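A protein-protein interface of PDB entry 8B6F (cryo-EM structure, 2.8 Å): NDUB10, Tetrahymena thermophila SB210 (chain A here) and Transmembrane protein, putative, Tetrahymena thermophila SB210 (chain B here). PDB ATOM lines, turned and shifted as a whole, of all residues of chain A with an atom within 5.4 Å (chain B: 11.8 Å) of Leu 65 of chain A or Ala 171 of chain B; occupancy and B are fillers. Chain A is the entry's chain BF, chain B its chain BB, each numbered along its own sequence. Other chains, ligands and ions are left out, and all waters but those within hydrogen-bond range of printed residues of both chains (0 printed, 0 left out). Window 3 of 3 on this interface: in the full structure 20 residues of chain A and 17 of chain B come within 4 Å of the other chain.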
ATOM      1  N   LEU A  60      -2.860  13.633 -20.240  1.00  0.00           N
ATOM      2  CA  LEU A  60      -2.643  14.420 -21.448  1.00  0.00           C
ATOM      3  C   LEU A  60      -3.430  13.852 -22.621  1.00  0.00           C
ATOM      4  O   LEU A  60      -4.050  14.603 -23.382  1.00  0.00           O
ATOM      5  CB  LEU A  60      -1.153  14.473 -21.782  1.00  0.00           C
ATOM      6  CG  LEU A  60      -0.769  15.247 -23.045  1.00  0.00           C
ATOM      7  CD1 LEU A  60      -1.137  16.717 -22.919  1.00  0.00           C
ATOM      8  CD2 LEU A  60       0.711  15.087 -23.326  1.00  0.00           C
ATOM      9  N   ARG A  61      -3.420  12.529 -22.785  1.00  0.00           N
ATOM     10  CA  ARG A  61      -4.198  11.911 -23.853  1.00  0.00           C
ATOM     11  C   ARG A  61      -5.684  12.194 -23.678  1.00  0.00           C
ATOM     12  O   ARG A  61      -6.382  12.536 -24.638  1.00  0.00           O
ATOM     13  CB  ARG A  61      -3.927  10.406 -23.880  1.00  0.00           C
ATOM     14  CG  ARG A  61      -4.959   9.591 -24.632  1.00  0.00           C
ATOM     15  CD  ARG A  61      -4.561   8.127 -24.682  1.00  0.00           C
ATOM     16  NE  ARG A  61      -5.706   7.275 -24.977  1.00  0.00           N
ATOM     17  CZ  ARG A  61      -6.521   6.769 -24.061  1.00  0.00           C
ATOM     18  NH1 ARG A  61      -6.338   6.992 -22.771  1.00  0.00           N
ATOM     19  NH2 ARG A  61      -7.551   6.022 -24.452  1.00  0.00           N
ATOM     20  N   ILE A  62      -6.189  12.046 -22.452  1.00  0.00           N
ATOM     21  CA  ILE A  62      -7.597  12.314 -22.187  1.00  0.00           C
ATOM     22  C   ILE A  62      -7.914  13.788 -22.400  1.00  0.00           C
ATOM     23  O   ILE A  62      -9.008  14.136 -22.859  1.00  0.00           O
ATOM     24  CB  ILE A  62      -7.974  11.852 -20.767  1.00  0.00           C
ATOM     25  CG1 ILE A  62      -7.810  10.335 -20.628  1.00  0.00           C
ATOM     26  CG2 ILE A  62      -9.404  12.259 -20.423  1.00  0.00           C
ATOM     27  CD1 ILE A  62      -8.590   9.514 -21.632  1.00  0.00           C
ATOM     28  N   GLY A  63      -6.971  14.675 -22.082  1.00  0.00           N
ATOM     29  CA  GLY A  63      -7.205  16.092 -22.301  1.00  0.00           C
ATOM     30  C   GLY A  63      -7.270  16.453 -23.771  1.00  0.00           C
ATOM     31  O   GLY A  63      -8.095  17.274 -24.177  1.00  0.00           O
ATOM     32  N   GLU A  64      -6.412  15.847 -24.590  1.00  0.00           N
ATOM     33  CA  GLU A  64      -6.519  16.052 -26.029  1.00  0.00           C
ATOM     34  C   GLU A  64      -7.868  15.564 -26.541  1.00  0.00           C
ATOM     35  O   GLU A  64      -8.531  16.244 -27.330  1.00  0.00           O
ATOM     36  CB  GLU A  64      -5.376  15.334 -26.745  1.00  0.00           C
ATOM     37  CG  GLU A  64      -3.991  15.834 -26.366  1.00  0.00           C
ATOM     38  CD  GLU A  64      -3.689  17.209 -26.923  1.00  0.00           C
ATOM     39  OE1 GLU A  64      -4.619  17.869 -27.431  1.00  0.00           O
ATOM     40  OE2 GLU A  64      -2.515  17.629 -26.860  1.00  0.00           O
ATOM     41  N   LEU A  65      -8.286  14.375 -26.102  1.00  0.00           N
ATOM     42  CA  LEU A  65      -9.607  13.873 -26.461  1.00  0.00           C
ATOM     43  C   LEU A  65     -10.708  14.791 -25.945  1.00  0.00           C
ATOM     44  O   LEU A  65     -11.761  14.916 -26.579  1.00  0.00           O
ATOM     45  CB  LEU A  65      -9.795  12.459 -25.914  1.00  0.00           C
ATOM     46  CG  LEU A  65      -8.882  11.384 -26.507  1.00  0.00           C
ATOM     47  CD1 LEU A  65      -9.028  10.081 -25.741  1.00  0.00           C
ATOM     48  CD2 LEU A  65      -9.182  11.169 -27.979  1.00  0.00           C
ATOM     49  N   PHE A  66     -10.486  15.430 -24.795  1.00  0.00           N
ATOM     50  CA  PHE A  66     -11.498  16.308 -24.217  1.00  0.00           C
ATOM     51  C   PHE A  66     -11.646  17.590 -25.026  1.00  0.00           C
ATOM     52  O   PHE A  66     -12.763  18.076 -25.230  1.00  0.00           O
ATOM     53  CB  PHE A  66     -11.132  16.623 -22.765  1.00  0.00           C
ATOM     54  CG  PHE A  66     -12.241  17.258 -21.980  1.00  0.00           C
ATOM     55  CD1 PHE A  66     -13.439  16.595 -21.780  1.00  0.00           C
ATOM     56  CD2 PHE A  66     -12.069  18.506 -21.411  1.00  0.00           C
ATOM     57  CE1 PHE A  66     -14.455  17.177 -21.047  1.00  0.00           C
ATOM     58  CE2 PHE A  66     -13.079  19.093 -20.676  1.00  0.00           C
ATOM     59  CZ  PHE A  66     -14.274  18.427 -20.494  1.00  0.00           C
ATOM     60  N   LEU A  67     -10.533  18.150 -25.496  1.00  0.00           N
ATOM     61  CA  LEU A  67     -10.606  19.308 -26.380  1.00  0.00           C
ATOM     62  C   LEU A  67     -11.268  18.947 -27.704  1.00  0.00           C
ATOM     63  O   LEU A  67     -12.078  19.719 -28.229  1.00  0.00           O
ATOM     64  CB  LEU A  67      -9.210  19.881 -26.604  1.00  0.00           C
ATOM     65  CG  LEU A  67      -8.460  20.324 -25.346  1.00  0.00           C
ATOM     66  CD1 LEU A  67      -7.073  20.819 -25.704  1.00  0.00           C
ATOM     67  CD2 LEU A  67      -9.231  21.396 -24.596  1.00  0.00           C
ATOM     68  N   ASN A  68     -10.936  17.783 -28.261  1.00  0.00           N
ATOM     69  CA  ASN A  68     -11.626  17.317 -29.459  1.00  0.00           C
ATOM     70  C   ASN A  68     -13.114  17.146 -29.190  1.00  0.00           C
ATOM     71  O   ASN A  68     -13.946  17.399 -30.067  1.00  0.00           O
ATOM     72  CB  ASN A  68     -11.017  16.005 -29.952  1.00  0.00           C
ATOM     73  CG  ASN A  68      -9.641  16.191 -30.553  1.00  0.00           C
ATOM     74  OD1 ASN A  68      -9.284  17.283 -30.988  1.00  0.00           O
ATOM     75  ND2 ASN A  68      -8.863  15.118 -30.589  1.00  0.00           N
ATOM     76  N   GLU A  69     -13.466  16.714 -27.978  1.00  0.00           N
ATOM     77  CA  GLU A  69     -14.872  16.582 -27.614  1.00  0.00           C
ATOM     78  C   GLU A  69     -15.548  17.944 -27.549  1.00  0.00           C
ATOM     79  O   GLU A  69     -16.707  18.086 -27.953  1.00  0.00           O
ATOM     80  CB  GLU A  69     -15.000  15.850 -26.277  1.00  0.00           C
ATOM     81  CG  GLU A  69     -16.432  15.506 -25.892  1.00  0.00           C
ATOM     82  CD  GLU A  69     -17.076  14.521 -26.848  1.00  0.00           C
ATOM     83  OE1 GLU A  69     -16.346  13.892 -27.642  1.00  0.00           O
ATOM     84  OE2 GLU A  69     -18.315  14.373 -26.807  1.00  0.00           O
ATOM     85  N   TYR A  70     -14.848  18.959 -27.038  1.00  0.00           N
ATOM     86  CA  TYR A  70     -15.383  20.315 -27.092  1.00  0.00           C
ATOM     87  C   TYR A  70     -15.689  20.718 -28.529  1.00  0.00           C
ATOM     88  O   TYR A  70     -16.752  21.277 -28.816  1.00  0.00           O
ATOM     89  CB  TYR A  70     -14.391  21.302 -26.471  1.00  0.00           C
ATOM     90  CG  TYR A  70     -14.447  21.418 -24.963  1.00  0.00           C
ATOM     91  CD1 TYR A  70     -15.322  20.646 -24.214  1.00  0.00           C
ATOM     92  CD2 TYR A  70     -13.640  22.326 -24.292  1.00  0.00           C
ATOM     93  CE1 TYR A  70     -15.379  20.760 -22.849  1.00  0.00           C
ATOM     94  CE2 TYR A  70     -13.692  22.446 -22.917  1.00  0.00           C
ATOM     95  CZ  TYR A  70     -14.570  21.658 -22.204  1.00  0.00           C
ATOM     96  OH  TYR A  70     -14.662  21.738 -20.836  1.00  0.00           O
ATOM     97  N   ARG A 111      -6.424  19.295 -31.495  1.00  0.00           N
ATOM     98  CA  ARG A 111      -5.862  18.425 -32.526  1.00  0.00           C
ATOM     99  C   ARG A 111      -6.993  17.569 -33.077  1.00  0.00           C
ATOM    100  O   ARG A 111      -7.292  16.490 -32.566  1.00  0.00           O
ATOM    101  CB  ARG A 111      -4.734  17.581 -31.952  1.00  0.00           C
ATOM    102  CG  ARG A 111      -4.137  16.560 -32.911  1.00  0.00           C
ATOM    103  CD  ARG A 111      -3.689  15.315 -32.165  1.00  0.00           C
ATOM    104  NE  ARG A 111      -4.814  14.619 -31.554  1.00  0.00           N
ATOM    105  CZ  ARG A 111      -4.702  13.663 -30.643  1.00  0.00           C
ATOM    106  NH1 ARG A 111      -3.522  13.265 -30.199  1.00  0.00           N
ATOM    107  NH2 ARG A 111      -5.803  13.089 -30.168  1.00  0.00           N
ATOM    108  N   ASN B 166     -20.575   0.137 -21.797  1.00  0.00           N
ATOM    109  CA  ASN B 166     -19.465   0.098 -20.849  1.00  0.00           C
ATOM    110  C   ASN B 166     -18.214   0.781 -21.391  1.00  0.00           C
ATOM    111  O   ASN B 166     -17.678   1.692 -20.753  1.00  0.00           O
ATOM    112  CB  ASN B 166     -19.163  -1.358 -20.470  1.00  0.00           C
ATOM    113  CG  ASN B 166     -20.287  -1.995 -19.676  1.00  0.00           C
ATOM    114  OD1 ASN B 166     -20.316  -1.916 -18.449  1.00  0.00           O
ATOM    115  ND2 ASN B 166     -21.222  -2.630 -20.376  1.00  0.00           N
ATOM    116  N   LEU B 167     -17.733   0.355 -22.554  1.00  0.00           N
ATOM    117  CA  LEU B 167     -16.539   0.949 -23.153  1.00  0.00           C
ATOM    118  C   LEU B 167     -16.958   2.193 -23.922  1.00  0.00           C
ATOM    119  O   LEU B 167     -17.252   2.149 -25.117  1.00  0.00           O
ATOM    120  CB  LEU B 167     -15.823  -0.054 -24.047  1.00  0.00           C
ATOM    121  CG  LEU B 167     -14.779  -0.921 -23.338  1.00  0.00           C
ATOM    122  CD1 LEU B 167     -15.380  -1.647 -22.150  1.00  0.00           C
ATOM    123  CD2 LEU B 167     -14.164  -1.910 -24.310  1.00  0.00           C
ATOM    124  N   ALA B 168     -16.988   3.321 -23.218  1.00  0.00           N
ATOM    125  CA  ALA B 168     -17.339   4.609 -23.791  1.00  0.00           C
ATOM    126  C   ALA B 168     -16.143   5.544 -23.704  1.00  0.00           C
ATOM    127  O   ALA B 168     -15.243   5.359 -22.881  1.00  0.00           O
ATOM    128  CB  ALA B 168     -18.546   5.229 -23.075  1.00  0.00           C
ATOM    129  N   ASN B 169     -16.144   6.554 -24.561  1.00  0.00           N
ATOM    130  CA  ASN B 169     -15.020   7.472 -24.635  1.00  0.00           C
ATOM    131  C   ASN B 169     -14.853   8.183 -23.296  1.00  0.00           C
ATOM    132  O   ASN B 169     -15.794   8.847 -22.838  1.00  0.00           O
ATOM    133  CB  ASN B 169     -15.246   8.488 -25.750  1.00  0.00           C
ATOM    134  CG  ASN B 169     -14.033   9.357 -26.003  1.00  0.00           C
ATOM    135  OD1 ASN B 169     -12.931   9.049 -25.554  1.00  0.00           O
ATOM    136  ND2 ASN B 169     -14.231  10.451 -26.727  1.00  0.00           N
ATOM    137  N   PRO B 170     -13.697   8.079 -22.638  1.00  0.00           N
ATOM    138  CA  PRO B 170     -13.523   8.805 -21.372  1.00  0.00           C
ATOM    139  C   PRO B 170     -13.709  10.304 -21.513  1.00  0.00           C
ATOM    140  O   PRO B 170     -14.197  10.949 -20.577  1.00  0.00           O
ATOM    141  CB  PRO B 170     -12.092   8.446 -20.956  1.00  0.00           C
ATOM    142  CG  PRO B 170     -11.812   7.159 -21.630  1.00  0.00           C
ATOM    143  CD  PRO B 170     -12.541   7.217 -22.936  1.00  0.00           C
ATOM    144  N   ALA B 171     -13.331  10.880 -22.655  1.00  0.00           N
ATOM    145  CA  ALA B 171     -13.506  12.314 -22.852  1.00  0.00           C
ATOM    146  C   ALA B 171     -14.980  12.692 -22.836  1.00  0.00           C
ATOM    147  O   ALA B 171     -15.375  13.666 -22.188  1.00  0.00           O
ATOM    148  CB  ALA B 171     -12.854  12.746 -24.165  1.00  0.00           C
ATOM    149  N   GLU B 172     -15.815  11.932 -23.548  1.00  0.00           N
ATOM    150  CA  GLU B 172     -17.238  12.252 -23.572  1.00  0.00           C
ATOM    151  C   GLU B 172     -17.874  11.993 -22.211  1.00  0.00           C
ATOM    152  O   GLU B 172     -18.761  12.740 -21.783  1.00  0.00           O
ATOM    153  CB  GLU B 172     -17.947  11.454 -24.668  1.00  0.00           C
ATOM    154  CG  GLU B 172     -18.441  10.082 -24.246  1.00  0.00           C
ATOM    155  CD  GLU B 172     -18.975   9.280 -25.413  1.00  0.00           C
ATOM    156  OE1 GLU B 172     -19.018   9.826 -26.535  1.00  0.00           O
ATOM    157  OE2 GLU B 172     -19.350   8.105 -25.211  1.00  0.00           O
ATOM    158  N   SER B 173     -17.440  10.937 -21.521  1.00  0.00           N
ATOM    159  CA  SER B 173     -17.930  10.696 -20.169  1.00  0.00           C
ATOM    160  C   SER B 173     -17.571  11.858 -19.256  1.00  0.00           C
ATOM    161  O   SER B 173     -18.403  12.326 -18.473  1.00  0.00           O
ATOM    162  CB  SER B 173     -17.354   9.392 -19.618  1.00  0.00           C
ATOM    163  OG  SER B 173     -17.751   8.284 -20.407  1.00  0.00           O
ATOM    164  N   LEU B 174     -16.335  12.348 -19.360  1.00  0.00           N
ATOM    165  CA  LEU B 174     -15.918  13.483 -18.548  1.00  0.00           C
ATOM    166  C   LEU B 174     -16.741  14.719 -18.876  1.00  0.00           C
ATOM    167  O   LEU B 174     -17.133  15.472 -17.977  1.00  0.00           O
ATOM    168  CB  LEU B 174     -14.430  13.756 -18.768  1.00  0.00           C
ATOM    169  CG  LEU B 174     -13.766  14.739 -17.803  1.00  0.00           C
ATOM    170  CD1 LEU B 174     -13.542  14.083 -16.456  1.00  0.00           C
ATOM    171  CD2 LEU B 174     -12.457  15.243 -18.380  1.00  0.00           C
ATOM    172  N   PHE B 175     -17.015  14.948 -20.162  1.00  0.00           N
ATOM    173  CA  PHE B 175     -17.826  16.095 -20.556  1.00  0.00           C
ATOM    174  C   PHE B 175     -19.224  16.012 -19.953  1.00  0.00           C
ATOM    175  O   PHE B 175     -19.740  16.998 -19.413  1.00  0.00           O
ATOM    176  CB  PHE B 175     -17.900  16.180 -22.082  1.00  0.00           C
ATOM    177  CG  PHE B 175     -18.585  17.416 -22.588  1.00  0.00           C
ATOM    178  CD1 PHE B 175     -19.955  17.440 -22.785  1.00  0.00           C
ATOM    179  CD2 PHE B 175     -17.854  18.556 -22.869  1.00  0.00           C
ATOM    180  CE1 PHE B 175     -20.580  18.580 -23.251  1.00  0.00           C
ATOM    181  CE2 PHE B 175     -18.472  19.696 -23.334  1.00  0.00           C
ATOM    182  CZ  PHE B 175     -19.836  19.709 -23.526  1.00  0.00           C
ATOM    183  N   SER B 176     -19.859  14.841 -20.042  1.00  0.00           N
ATOM    184  CA  SER B 176     -21.201  14.685 -19.490  1.00  0.00           C
ATOM    185  C   SER B 176     -21.209  14.882 -17.979  1.00  0.00           C
ATOM    186  O   SER B 176     -22.103  15.540 -17.435  1.00  0.00           O
ATOM    187  CB  SER B 176     -21.755  13.306 -19.844  1.00  0.00           C
ATOM    188  OG  SER B 176     -21.772  13.110 -21.246  1.00  0.00           O
ATOM    189  N   LEU B 177     -20.226  14.310 -17.282  1.00  0.00           N
ATOM    190  CA  LEU B 177     -20.173  14.454 -15.831  1.00  0.00           C
ATOM    191  C   LEU B 177     -19.922  15.902 -15.430  1.00  0.00           C
ATOM    192  O   LEU B 177     -20.490  16.384 -14.444  1.00  0.00           O
ATOM    193  CB  LEU B 177     -19.099  13.536 -15.249  1.00  0.00           C
ATOM    194  CG  LEU B 177     -19.335  12.031 -15.422  1.00  0.00           C
ATOM    195  CD1 LEU B 177     -18.260  11.238 -14.700  1.00  0.00           C
ATOM    196  CD2 LEU B 177     -20.724  11.604 -14.953  1.00  0.00           C
ATOM    197  N   ASN B 178     -19.076  16.611 -16.180  1.00  0.00           N
ATOM    198  CA  ASN B 178     -18.845  18.020 -15.887  1.00  0.00           C
ATOM    199  C   ASN B 178     -20.110  18.840 -16.104  1.00  0.00           C
ATOM    200  O   ASN B 178     -20.406  19.751 -15.322  1.00  0.00           O
ATOM    201  CB  ASN B 178     -17.702  18.557 -16.745  1.00  0.00           C
ATOM    202  CG  ASN B 178     -17.457  20.034 -16.524  1.00  0.00           C
ATOM    203  OD1 ASN B 178     -17.905  20.872 -17.304  1.00  0.00           O
ATOM    204  ND2 ASN B 178     -16.752  20.363 -15.447  1.00  0.00           N
ATOM    205  N   THR B 179     -20.866  18.539 -17.159  1.00  0.00           N
ATOM    206  CA  THR B 179     -22.138  19.222 -17.362  1.00  0.00           C
ATOM    207  C   THR B 179     -23.078  18.966 -16.192  1.00  0.00           C
ATOM    208  O   THR B 179     -23.745  19.886 -15.706  1.00  0.00           O
ATOM    209  CB  THR B 179     -22.780  18.761 -18.671  1.00  0.00           C
ATOM    210  OG1 THR B 179     -21.844  18.909 -19.746  1.00  0.00           O
ATOM    211  CG2 THR B 179     -24.023  19.581 -18.977  1.00  0.00           C
ATOM    212  N   ALA B 180     -23.145  17.718 -15.729  1.00  0.00           N
ATOM    213  CA  ALA B 180     -23.989  17.395 -14.584  1.00  0.00           C
ATOM    214  C   ALA B 180     -23.540  18.151 -13.341  1.00  0.00           C
ATOM    215  O   ALA B 180     -24.371  18.650 -12.574  1.00  0.00           O
ATOM    216  CB  ALA B 180     -23.975  15.889 -14.331  1.00  0.00           C
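Of the 15 printed residues of chain B, 5 touch a printed residue of chain A. Printed residues of chain B that touch a printed residue of chain A: Pro 170, Ala 171, Glu 172, Leu 174 and Phe 175. Hydrophobic or aromatic side chains of chain B that line the printed part of chain A: Pro 170, Ala 171, Leu 174 and Phe 175. Of the 12 printed residues of chain A, 5 touch a printed residue of chain B. Hydrophobic or aromatic side chains of chain A that line the printed part of chain B: Ile 62, Leu 65, Phe 66 and Tyr 70. Along chain A the printed residues that touch a printed residue of chain B span positions 62 to 70. Among the printed residues, no Asp or Glu carboxylate lies within 4 Å of a Lys or Arg side-chain nitrogen of the other chain.
CD1 of Ile 62 of chain A touches CB of Pro 170 of chain B (3.7 Å). CB of Ala 171 of chain B touches O of Leu 65 of chain A (3.4 Å). CD1 of Phe 66 of chain A touches O of Ala 171 of chain B, at 3.5 Å. Phe 66 of chain A touches Leu 174 of chain B (CD1 to CD2, 3.8 Å). CE1 of Phe 66 of chain A touches N of Phe 175 of chain B, 3.5 Å away. Glu 172 of chain B touches Glu 69 of chain A. Tyr 70 of chain A touches Phe 175 of chain B.
Printed residues of chain B within 4 Å of Leu 65 of chain A: Ala 171 (3.4 Å). Of the printed residues of chain A, Ala 171 of chain B touches Leu 65 (3.4 Å) and Phe 66 (3.5 Å). No residue of chain B comes within 4 Å of Arg 61 of chain A. Ile 62 of chain A touches just one residue of chain B: Pro 170 (3.7 Å). No residue of chain B comes within 4 Å of Gly 63 of chain A. No residue of chain B comes within 4 Å of Glu 64 of chain A. Phe 66 of chain A touches just these residues of chain B: Ala 171, Leu 174 and Phe 175. Leu 67 of chain A touches none of the printed residues of chain B. Asn 68 of chain A touches none of the printed residues of chain B. Glu 69 of chain A touches just one residue of chain B: Glu 172 (3.6 Å). Of the printed residues of chain A, Phe 175 of chain B touches Phe 66 (3.5 Å) and Tyr 70 (3.3 Å). Printed residues of chain A within 4 Å of Leu 174 of chain B: Phe 66 (3.8 Å). Ala 168 of chain B touches none of the printed residues of chain A. Asn 169 of chain B touches none of the printed residues of chain A. The nearest residue of chain B that does not touch Leu 65 of chain A is Asn 169 of chain B (4.04 Å). The nearest printed residue of chain A that does not touch Ala 171 of chain B is Glu 69 of chain A (4.3 Å).
OD1 of Asn 169 of chain B lies close to N of Ala 171 of chain B (3.5 Å). The backbone carbonyl oxygen (O) of Glu 172 of chain B lies within hydrogen-bond range of the side-chain hydroxyl (OG) of Ser 176 of chain B (3.1 Å). The side-chain hydroxyl (OG1) of Thr 179 of chain B is in hydrogen-bond range of the backbone carbonyl oxygen (O) of Phe 175 of chain B, 2.9 Å away.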
